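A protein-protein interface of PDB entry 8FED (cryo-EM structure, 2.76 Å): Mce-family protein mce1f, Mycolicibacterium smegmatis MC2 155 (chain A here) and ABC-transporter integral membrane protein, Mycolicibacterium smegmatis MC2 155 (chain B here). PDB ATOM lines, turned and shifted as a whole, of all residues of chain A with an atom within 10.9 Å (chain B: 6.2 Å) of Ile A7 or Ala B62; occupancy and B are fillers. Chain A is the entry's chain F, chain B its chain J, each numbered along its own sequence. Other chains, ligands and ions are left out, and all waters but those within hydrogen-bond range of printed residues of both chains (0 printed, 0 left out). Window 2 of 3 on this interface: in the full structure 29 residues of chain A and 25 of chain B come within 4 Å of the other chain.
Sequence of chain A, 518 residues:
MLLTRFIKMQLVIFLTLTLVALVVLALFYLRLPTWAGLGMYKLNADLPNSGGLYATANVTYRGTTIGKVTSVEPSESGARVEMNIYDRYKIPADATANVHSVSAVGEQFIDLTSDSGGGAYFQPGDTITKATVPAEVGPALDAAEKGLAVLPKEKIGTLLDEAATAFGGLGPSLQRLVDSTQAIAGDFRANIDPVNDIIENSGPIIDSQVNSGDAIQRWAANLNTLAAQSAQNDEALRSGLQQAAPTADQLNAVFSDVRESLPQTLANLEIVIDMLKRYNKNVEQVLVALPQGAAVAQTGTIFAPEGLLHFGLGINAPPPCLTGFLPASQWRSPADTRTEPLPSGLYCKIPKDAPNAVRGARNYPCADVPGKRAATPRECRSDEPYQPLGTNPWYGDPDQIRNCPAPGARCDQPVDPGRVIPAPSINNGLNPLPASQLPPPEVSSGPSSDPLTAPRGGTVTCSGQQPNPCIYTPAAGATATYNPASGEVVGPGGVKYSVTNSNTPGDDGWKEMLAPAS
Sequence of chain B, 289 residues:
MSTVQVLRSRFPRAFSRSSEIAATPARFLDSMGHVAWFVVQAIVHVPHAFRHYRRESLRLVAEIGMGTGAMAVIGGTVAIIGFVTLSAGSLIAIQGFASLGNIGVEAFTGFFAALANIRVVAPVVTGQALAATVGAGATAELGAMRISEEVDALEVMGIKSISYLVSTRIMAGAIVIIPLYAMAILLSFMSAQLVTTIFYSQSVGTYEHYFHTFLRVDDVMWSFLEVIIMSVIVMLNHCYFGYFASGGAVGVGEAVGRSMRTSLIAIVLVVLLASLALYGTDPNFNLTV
OE1 of Gln A10 sits close to O of Ala B62 (3.3 Å).
OE1 of Glu B63 is in salt-bridge range of NH1 of Arg B59. The backbone NH (N) of Ile A7 lies within hydrogen-bond range of the side-chain hydroxyl (OG1) of Thr A4.
CD2 of Leu A2 touches CB of Arg B59 (3.7 Å). CA of Arg B59 touches CG2 of Ile A7, at 3.8 Å. Ile A7 touches Ala B62 (CG2 to CB, 3.7 Å). Met B66 touches Gln A10 (CB to OE1, 3.5 Å). CD1 of Leu A11 touches O of Leu B58 (3.9 Å). Leu A11 touches Val B61. Ala B62 touches Leu A11 (N to CD1, 3.9 Å).
Of the printed residues of chain B, Ile A7 touches Arg B59 and Ala B62. Ala B62 touches just these residues of chain A: Ile A7 (3.7 Å), Gln A10 (3.3 Å) and Leu A11 (3.9 Å). Val B61 touches just one residue of chain A: Leu A11 (3.7 Å). Of the printed residues of chain A, Arg B59 touches Leu A2 (3.7 Å) and Ile A7 (3.8 Å). Printed residues of chain B within 4 Å of Leu A11: Leu B58 (3.9 Å), Val B61 (3.7 Å) and Ala B62 (3.9 Å). Of the printed residues of chain B, Gln A10 touches Ala B62 and Met B66. Printed residues of chain B within 4 Å of Leu A2: Arg B59 (3.7 Å). Of the printed residues of chain A, Leu B58 touches Leu A11. The nearest residue of chain B that does not touch Ile A7 is Leu B58 (4.5 Å). The nearest residue of chain A that does not touch Ala B62 is Lys A8 (5.7 Å). The nearest printed residue of chain B that does not touch Leu A11 is Met B66 (5.4 Å).
Printed residues of chain A that touch a printed residue of chain B: Leu A2, Ile A7, Gln A10 and Leu A11. Among the printed residues, 8 pairs touch across the chains. Among the printed residues, no Asp or Glu carboxylate lies within 4 Å of a Lys or Arg side-chain nitrogen of the other chain.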
ATOM      1  N   MET A   1       9.685  -8.662  11.264  1.00  0.00           N
ATOM      2  CA  MET A   1      10.362  -8.085  10.108  1.00  0.00           C
ATOM      3  C   MET A   1       9.690  -6.791   9.666  1.00  0.00           C
ATOM      4  O   MET A   1       8.481  -6.770   9.426  1.00  0.00           O
ATOM      5  CB  MET A   1      10.390  -9.086   8.951  1.00  0.00           C
ATOM      6  CG  MET A   1      10.885  -8.510   7.635  1.00  0.00           C
ATOM      7  SD  MET A   1      12.574  -7.885   7.718  1.00  0.00           S
ATOM      8  CE  MET A   1      12.801  -7.306   6.038  1.00  0.00           C
ATOM      9  N   LEU A   2      10.486  -5.729   9.559  1.00  0.00           N
ATOM     10  CA  LEU A   2      10.046  -4.407   9.083  1.00  0.00           C
ATOM     11  C   LEU A   2       8.929  -3.930  10.012  1.00  0.00           C
ATOM     12  O   LEU A   2       9.151  -3.890  11.234  1.00  0.00           O
ATOM     13  CB  LEU A   2       9.689  -4.509   7.602  1.00  0.00           C
ATOM     14  CG  LEU A   2       9.533  -3.222   6.792  1.00  0.00           C
ATOM     15  CD1 LEU A   2      10.864  -2.498   6.671  1.00  0.00           C
ATOM     16  CD2 LEU A   2       8.962  -3.542   5.425  1.00  0.00           C
ATOM     17  N   LEU A   3       7.753  -3.558   9.496  1.00  0.00           N
ATOM     18  CA  LEU A   3       6.623  -3.072  10.291  1.00  0.00           C
ATOM     19  C   LEU A   3       7.000  -1.828  11.101  1.00  0.00           C
ATOM     20  O   LEU A   3       6.887  -1.790  12.329  1.00  0.00           O
ATOM     21  CB  LEU A   3       6.066  -4.176  11.198  1.00  0.00           C
ATOM     22  CG  LEU A   3       5.504  -5.413  10.499  1.00  0.00           C
ATOM     23  CD1 LEU A   3       4.961  -6.400  11.521  1.00  0.00           C
ATOM     24  CD2 LEU A   3       4.426  -5.026   9.499  1.00  0.00           C
ATOM     25  N   THR A   4       7.455  -0.799  10.381  1.00  0.00           N
ATOM     26  CA  THR A   4       7.860   0.443  11.031  1.00  0.00           C
ATOM     27  C   THR A   4       6.673   1.209  11.597  1.00  0.00           C
ATOM     28  O   THR A   4       6.869   2.083  12.448  1.00  0.00           O
ATOM     29  CB  THR A   4       8.620   1.332  10.045  1.00  0.00           C
ATOM     30  OG1 THR A   4       7.726   1.780   9.019  1.00  0.00           O
ATOM     31  CG2 THR A   4       9.766   0.563   9.405  1.00  0.00           C
ATOM     32  N   ARG A   5       5.465   0.930  11.093  1.00  0.00           N
ATOM     33  CA  ARG A   5       4.190   1.542  11.464  1.00  0.00           C
ATOM     34  C   ARG A   5       4.053   2.970  10.945  1.00  0.00           C
ATOM     35  O   ARG A   5       2.986   3.578  11.078  1.00  0.00           O
ATOM     36  CB  ARG A   5       3.965   1.501  12.981  1.00  0.00           C
ATOM     37  CG  ARG A   5       3.777   0.098  13.534  1.00  0.00           C
ATOM     38  CD  ARG A   5       3.143   0.132  14.913  1.00  0.00           C
ATOM     39  NE  ARG A   5       1.876   0.851  14.906  1.00  0.00           N
ATOM     40  CZ  ARG A   5       0.692   0.283  14.722  1.00  0.00           C
ATOM     41  NH1 ARG A   5       0.572  -1.022  14.538  1.00  0.00           N
ATOM     42  NH2 ARG A   5      -0.400   1.042  14.724  1.00  0.00           N
ATOM     43  N   PHE A   6       5.115   3.518  10.355  1.00  0.00           N
ATOM     44  CA  PHE A   6       4.966   4.709   9.530  1.00  0.00           C
ATOM     45  C   PHE A   6       4.642   4.332   8.092  1.00  0.00           C
ATOM     46  O   PHE A   6       3.813   4.983   7.444  1.00  0.00           O
ATOM     47  CB  PHE A   6       6.239   5.557   9.588  1.00  0.00           C
ATOM     48  CG  PHE A   6       6.151   6.838   8.808  1.00  0.00           C
ATOM     49  CD1 PHE A   6       5.553   7.958   9.360  1.00  0.00           C
ATOM     50  CD2 PHE A   6       6.681   6.928   7.531  1.00  0.00           C
ATOM     51  CE1 PHE A   6       5.474   9.142   8.649  1.00  0.00           C
ATOM     52  CE2 PHE A   6       6.606   8.107   6.817  1.00  0.00           C
ATOM     53  CZ  PHE A   6       6.001   9.215   7.376  1.00  0.00           C
ATOM     54  N   ILE A   7       5.289   3.276   7.593  1.00  0.00           N
ATOM     55  CA  ILE A   7       4.879   2.659   6.336  1.00  0.00           C
ATOM     56  C   ILE A   7       3.439   2.174   6.438  1.00  0.00           C
ATOM     57  O   ILE A   7       2.658   2.299   5.488  1.00  0.00           O
ATOM     58  CB  ILE A   7       5.847   1.519   5.969  1.00  0.00           C
ATOM     59  CG1 ILE A   7       7.209   2.086   5.563  1.00  0.00           C
ATOM     60  CG2 ILE A   7       5.280   0.647   4.863  1.00  0.00           C
ATOM     61  CD1 ILE A   7       7.159   2.968   4.338  1.00  0.00           C
ATOM     62  N   LYS A   8       3.062   1.632   7.599  1.00  0.00           N
ATOM     63  CA  LYS A   8       1.678   1.222   7.819  1.00  0.00           C
ATOM     64  C   LYS A   8       0.732   2.416   7.772  1.00  0.00           C
ATOM     65  O   LYS A   8      -0.375   2.319   7.228  1.00  0.00           O
ATOM     66  CB  LYS A   8       1.556   0.490   9.155  1.00  0.00           C
ATOM     67  CG  LYS A   8       0.251  -0.264   9.343  1.00  0.00           C
ATOM     68  CD  LYS A   8       0.134  -1.406   8.344  1.00  0.00           C
ATOM     69  CE  LYS A   8      -1.062  -2.293   8.644  1.00  0.00           C
ATOM     70  NZ  LYS A   8      -2.345  -1.543   8.596  1.00  0.00           N
ATOM     71  N   MET A   9       1.141   3.548   8.354  1.00  0.00           N
ATOM     72  CA  MET A   9       0.315   4.753   8.308  1.00  0.00           C
ATOM     73  C   MET A   9       0.132   5.242   6.877  1.00  0.00           C
ATOM     74  O   MET A   9      -0.981   5.592   6.460  1.00  0.00           O
ATOM     75  CB  MET A   9       0.940   5.846   9.176  1.00  0.00           C
ATOM     76  CG  MET A   9       0.282   7.208   9.029  1.00  0.00           C
ATOM     77  SD  MET A   9       1.150   8.502   9.936  1.00  0.00           S
ATOM     78  CE  MET A   9       0.192   9.942   9.473  1.00  0.00           C
ATOM     79  N   GLN A  10       1.224   5.271   6.105  1.00  0.00           N
ATOM     80  CA  GLN A  10       1.117   5.645   4.699  1.00  0.00           C
ATOM     81  C   GLN A  10       0.212   4.682   3.946  1.00  0.00           C
ATOM     82  O   GLN A  10      -0.601   5.103   3.116  1.00  0.00           O
ATOM     83  CB  GLN A  10       2.502   5.689   4.054  1.00  0.00           C
ATOM     84  CG  GLN A  10       3.356   6.869   4.474  1.00  0.00           C
ATOM     85  CD  GLN A  10       4.607   7.005   3.628  1.00  0.00           C
ATOM     86  OE1 GLN A  10       4.901   6.149   2.794  1.00  0.00           O
ATOM     87  NE2 GLN A  10       5.345   8.090   3.832  1.00  0.00           N
ATOM     88  N   LEU A  11       0.330   3.386   4.235  1.00  0.00           N
ATOM     89  CA  LEU A  11      -0.487   2.389   3.556  1.00  0.00           C
ATOM     90  C   LEU A  11      -1.967   2.580   3.860  1.00  0.00           C
ATOM     91  O   LEU A  11      -2.803   2.521   2.953  1.00  0.00           O
ATOM     92  CB  LEU A  11      -0.029   0.987   3.958  1.00  0.00           C
ATOM     93  CG  LEU A  11      -0.244  -0.126   2.936  1.00  0.00           C
ATOM     94  CD1 LEU A  11       0.511   0.190   1.661  1.00  0.00           C
ATOM     95  CD2 LEU A  11       0.202  -1.461   3.504  1.00  0.00           C
ATOM     96  N   VAL A  12      -2.313   2.819   5.128  1.00  0.00           N
ATOM     97  CA  VAL A  12      -3.726   2.943   5.479  1.00  0.00           C
ATOM     98  C   VAL A  12      -4.313   4.243   4.932  1.00  0.00           C
ATOM     99  O   VAL A  12      -5.460   4.263   4.466  1.00  0.00           O
ATOM    100  CB  VAL A  12      -3.948   2.794   7.000  1.00  0.00           C
ATOM    101  CG1 VAL A  12      -3.499   1.419   7.466  1.00  0.00           C
ATOM    102  CG2 VAL A  12      -3.249   3.882   7.792  1.00  0.00           C
ATOM    103  N   ILE A  13      -3.552   5.345   4.966  1.00  0.00           N
ATOM    104  CA  ILE A  13      -4.092   6.585   4.410  1.00  0.00           C
ATOM    105  C   ILE A  13      -4.227   6.475   2.892  1.00  0.00           C
ATOM    106  O   ILE A  13      -5.199   6.971   2.304  1.00  0.00           O
ATOM    107  CB  ILE A  13      -3.255   7.809   4.841  1.00  0.00           C
ATOM    108  CG1 ILE A  13      -3.954   9.103   4.421  1.00  0.00           C
ATOM    109  CG2 ILE A  13      -1.853   7.783   4.262  1.00  0.00           C
ATOM    110  CD1 ILE A  13      -3.180  10.358   4.763  1.00  0.00           C
ATOM    111  N   PHE A  14      -3.278   5.797   2.234  1.00  0.00           N
ATOM    112  CA  PHE A  14      -3.391   5.574   0.800  1.00  0.00           C
ATOM    113  C   PHE A  14      -4.591   4.696   0.472  1.00  0.00           C
ATOM    114  O   PHE A  14      -5.284   4.935  -0.520  1.00  0.00           O
ATOM    115  CB  PHE A  14      -2.103   4.951   0.261  1.00  0.00           C
ATOM    116  CG  PHE A  14      -2.214   4.461  -1.152  1.00  0.00           C
ATOM    117  CD1 PHE A  14      -2.161   5.350  -2.212  1.00  0.00           C
ATOM    118  CD2 PHE A  14      -2.368   3.112  -1.424  1.00  0.00           C
ATOM    119  CE1 PHE A  14      -2.266   4.904  -3.513  1.00  0.00           C
ATOM    120  CE2 PHE A  14      -2.473   2.660  -2.724  1.00  0.00           C
ATOM    121  CZ  PHE A  14      -2.424   3.558  -3.767  1.00  0.00           C
ATOM    122  N   LEU A  15      -4.851   3.673   1.290  1.00  0.00           N
ATOM    123  CA  LEU A  15      -6.009   2.816   1.060  1.00  0.00           C
ATOM    124  C   LEU A  15      -7.315   3.581   1.248  1.00  0.00           C
ATOM    125  O   LEU A  15      -8.268   3.387   0.485  1.00  0.00           O
ATOM    126  CB  LEU A  15      -5.959   1.603   1.989  1.00  0.00           C
ATOM    127  CG  LEU A  15      -7.092   0.589   1.822  1.00  0.00           C
ATOM    128  CD1 LEU A  15      -7.120   0.048   0.403  1.00  0.00           C
ATOM    129  CD2 LEU A  15      -6.955  -0.542   2.827  1.00  0.00           C
ATOM    130  N   THR A  16      -7.381   4.440   2.268  1.00  0.00           N
ATOM    131  CA  THR A  16      -8.574   5.258   2.474  1.00  0.00           C
ATOM    132  C   THR A  16      -8.816   6.180   1.284  1.00  0.00           C
ATOM    133  O   THR A  16      -9.939   6.270   0.767  1.00  0.00           O
ATOM    134  CB  THR A  16      -8.435   6.069   3.765  1.00  0.00           C
ATOM    135  OG1 THR A  16      -8.419   5.182   4.890  1.00  0.00           O
ATOM    136  CG2 THR A  16      -9.592   7.046   3.913  1.00  0.00           C
ATOM    137  N   THR A  18      -7.710   5.760  -1.737  1.00  0.00           N
ATOM    138  CA  THR A  18      -8.040   4.894  -2.862  1.00  0.00           C
ATOM    139  C   THR A  18      -9.517   4.533  -2.866  1.00  0.00           C
ATOM    140  O   THR A  18     -10.190   4.647  -3.896  1.00  0.00           O
ATOM    141  CB  THR A  18      -7.189   3.625  -2.796  1.00  0.00           C
ATOM    142  OG1 THR A  18      -5.833   3.935  -3.134  1.00  0.00           O
ATOM    143  CG2 THR A  18      -7.730   2.558  -3.740  1.00  0.00           C
ATOM    144  N   SER B  57       7.026  -5.898  -0.740  1.00  0.00           N
ATOM    145  CA  SER B  57       6.045  -5.393  -1.694  1.00  0.00           C
ATOM    146  C   SER B  57       5.141  -4.348  -1.055  1.00  0.00           C
ATOM    147  O   SER B  57       4.853  -3.316  -1.667  1.00  0.00           O
ATOM    148  CB  SER B  57       5.218  -6.543  -2.262  1.00  0.00           C
ATOM    149  OG  SER B  57       6.029  -7.426  -3.017  1.00  0.00           O
ATOM    150  N   LEU B  58       4.689  -4.593   0.176  1.00  0.00           N
ATOM    151  CA  LEU B  58       3.841  -3.616   0.853  1.00  0.00           C
ATOM    152  C   LEU B  58       4.603  -2.330   1.151  1.00  0.00           C
ATOM    153  O   LEU B  58       4.058  -1.227   1.002  1.00  0.00           O
ATOM    154  CB  LEU B  58       3.270  -4.214   2.138  1.00  0.00           C
ATOM    155  CG  LEU B  58       2.382  -5.447   1.966  1.00  0.00           C
ATOM    156  CD1 LEU B  58       1.799  -5.882   3.300  1.00  0.00           C
ATOM    157  CD2 LEU B  58       1.278  -5.178   0.956  1.00  0.00           C
ATOM    158  N   ARG B  59       5.863  -2.452   1.579  1.00  0.00           N
ATOM    159  CA  ARG B  59       6.668  -1.262   1.839  1.00  0.00           C
ATOM    160  C   ARG B  59       6.871  -0.450   0.568  1.00  0.00           C
ATOM    161  O   ARG B  59       6.784   0.783   0.590  1.00  0.00           O
ATOM    162  CB  ARG B  59       8.015  -1.651   2.442  1.00  0.00           C
ATOM    163  CG  ARG B  59       8.829  -0.461   2.919  1.00  0.00           C
ATOM    164  CD  ARG B  59      10.257  -0.852   3.249  1.00  0.00           C
ATOM    165  NE  ARG B  59      10.966  -1.362   2.082  1.00  0.00           N
ATOM    166  CZ  ARG B  59      11.577  -0.597   1.188  1.00  0.00           C
ATOM    167  NH1 ARG B  59      11.576   0.722   1.291  1.00  0.00           N
ATOM    168  NH2 ARG B  59      12.206  -1.169   0.166  1.00  0.00           N
ATOM    169  N   LEU B  60       7.136  -1.122  -0.556  1.00  0.00           N
ATOM    170  CA  LEU B  60       7.295  -0.408  -1.817  1.00  0.00           C
ATOM    171  C   LEU B  60       5.981   0.192  -2.298  1.00  0.00           C
ATOM    172  O   LEU B  60       5.988   1.257  -2.919  1.00  0.00           O
ATOM    173  CB  LEU B  60       7.888  -1.324  -2.885  1.00  0.00           C
ATOM    174  CG  LEU B  60       9.365  -1.657  -2.689  1.00  0.00           C
ATOM    175  CD1 LEU B  60       9.913  -2.375  -3.902  1.00  0.00           C
ATOM    176  CD2 LEU B  60      10.157  -0.392  -2.416  1.00  0.00           C
ATOM    177  N   VAL B  61       4.854  -0.471  -2.032  1.00  0.00           N
ATOM    178  CA  VAL B  61       3.554   0.110  -2.364  1.00  0.00           C
ATOM    179  C   VAL B  61       3.360   1.416  -1.611  1.00  0.00           C
ATOM    180  O   VAL B  61       2.966   2.436  -2.189  1.00  0.00           O
ATOM    181  CB  VAL B  61       2.421  -0.889  -2.063  1.00  0.00           C
ATOM    182  CG1 VAL B  61       1.085  -0.172  -1.986  1.00  0.00           C
ATOM    183  CG2 VAL B  61       2.367  -1.962  -3.127  1.00  0.00           C
ATOM    184  N   ALA B  62       3.649   1.406  -0.308  1.00  0.00           N
ATOM    185  CA  ALA B  62       3.524   2.627   0.484  1.00  0.00           C
ATOM    186  C   ALA B  62       4.485   3.704  -0.008  1.00  0.00           C
ATOM    187  O   ALA B  62       4.112   4.880  -0.110  1.00  0.00           O
ATOM    188  CB  ALA B  62       3.766   2.325   1.960  1.00  0.00           C
ATOM    189  N   GLU B  63       5.726   3.319  -0.316  1.00  0.00           N
ATOM    190  CA  GLU B  63       6.725   4.285  -0.763  1.00  0.00           C
ATOM    191  C   GLU B  63       6.341   4.917  -2.095  1.00  0.00           C
ATOM    192  O   GLU B  63       6.492   6.129  -2.280  1.00  0.00           O
ATOM    193  CB  GLU B  63       8.092   3.606  -0.866  1.00  0.00           C
ATOM    194  CG  GLU B  63       9.209   4.518  -1.342  1.00  0.00           C
ATOM    195  CD  GLU B  63      10.539   3.799  -1.449  1.00  0.00           C
ATOM    196  OE1 GLU B  63      10.609   2.616  -1.056  1.00  0.00           O
ATOM    197  OE2 GLU B  63      11.513   4.414  -1.930  1.00  0.00           O
ATOM    198  N   ILE B  64       5.849   4.113  -3.038  1.00  0.00           N
ATOM    199  CA  ILE B  64       5.441   4.644  -4.335  1.00  0.00           C
ATOM    200  C   ILE B  64       4.202   5.517  -4.190  1.00  0.00           C
ATOM    201  O   ILE B  64       4.115   6.596  -4.790  1.00  0.00           O
ATOM    202  CB  ILE B  64       5.219   3.494  -5.334  1.00  0.00           C
ATOM    203  CG1 ILE B  64       6.548   2.814  -5.666  1.00  0.00           C
ATOM    204  CG2 ILE B  64       4.555   4.000  -6.599  1.00  0.00           C
ATOM    205  CD1 ILE B  64       6.420   1.682  -6.658  1.00  0.00           C
ATOM    206  N   GLY B  65       3.228   5.077  -3.390  1.00  0.00           N
ATOM    207  CA  GLY B  65       2.008   5.850  -3.236  1.00  0.00           C
ATOM    208  C   GLY B  65       2.229   7.189  -2.559  1.00  0.00           C
ATOM    209  O   GLY B  65       1.687   8.207  -2.995  1.00  0.00           O
ATOM    210  N   MET B  66       3.030   7.214  -1.494  1.00  0.00           N
ATOM    211  CA  MET B  66       3.214   8.427  -0.707  1.00  0.00           C
ATOM    212  C   MET B  66       4.599   9.043  -0.882  1.00  0.00           C
ATOM    213  O   MET B  66       5.006   9.880  -0.071  1.00  0.00           O
ATOM    214  CB  MET B  66       2.933   8.143   0.767  1.00  0.00           C
ATOM    215  CG  MET B  66       1.589   7.478   1.010  1.00  0.00           C
ATOM    216  SD  MET B  66       0.229   8.324   0.182  1.00  0.00           S
ATOM    217  CE  MET B  66       0.259   9.913   1.005  1.00  0.00           C
ATOM    218  N   GLY B  67       5.331   8.646  -1.917  1.00  0.00           N
ATOM    219  CA  GLY B  67       6.601   9.274  -2.228  1.00  0.00           C
ATOM    220  C   GLY B  67       7.710   8.869  -1.273  1.00  0.00           C
ATOM    221  O   GLY B  67       7.547   8.045  -0.375  1.00  0.00           O
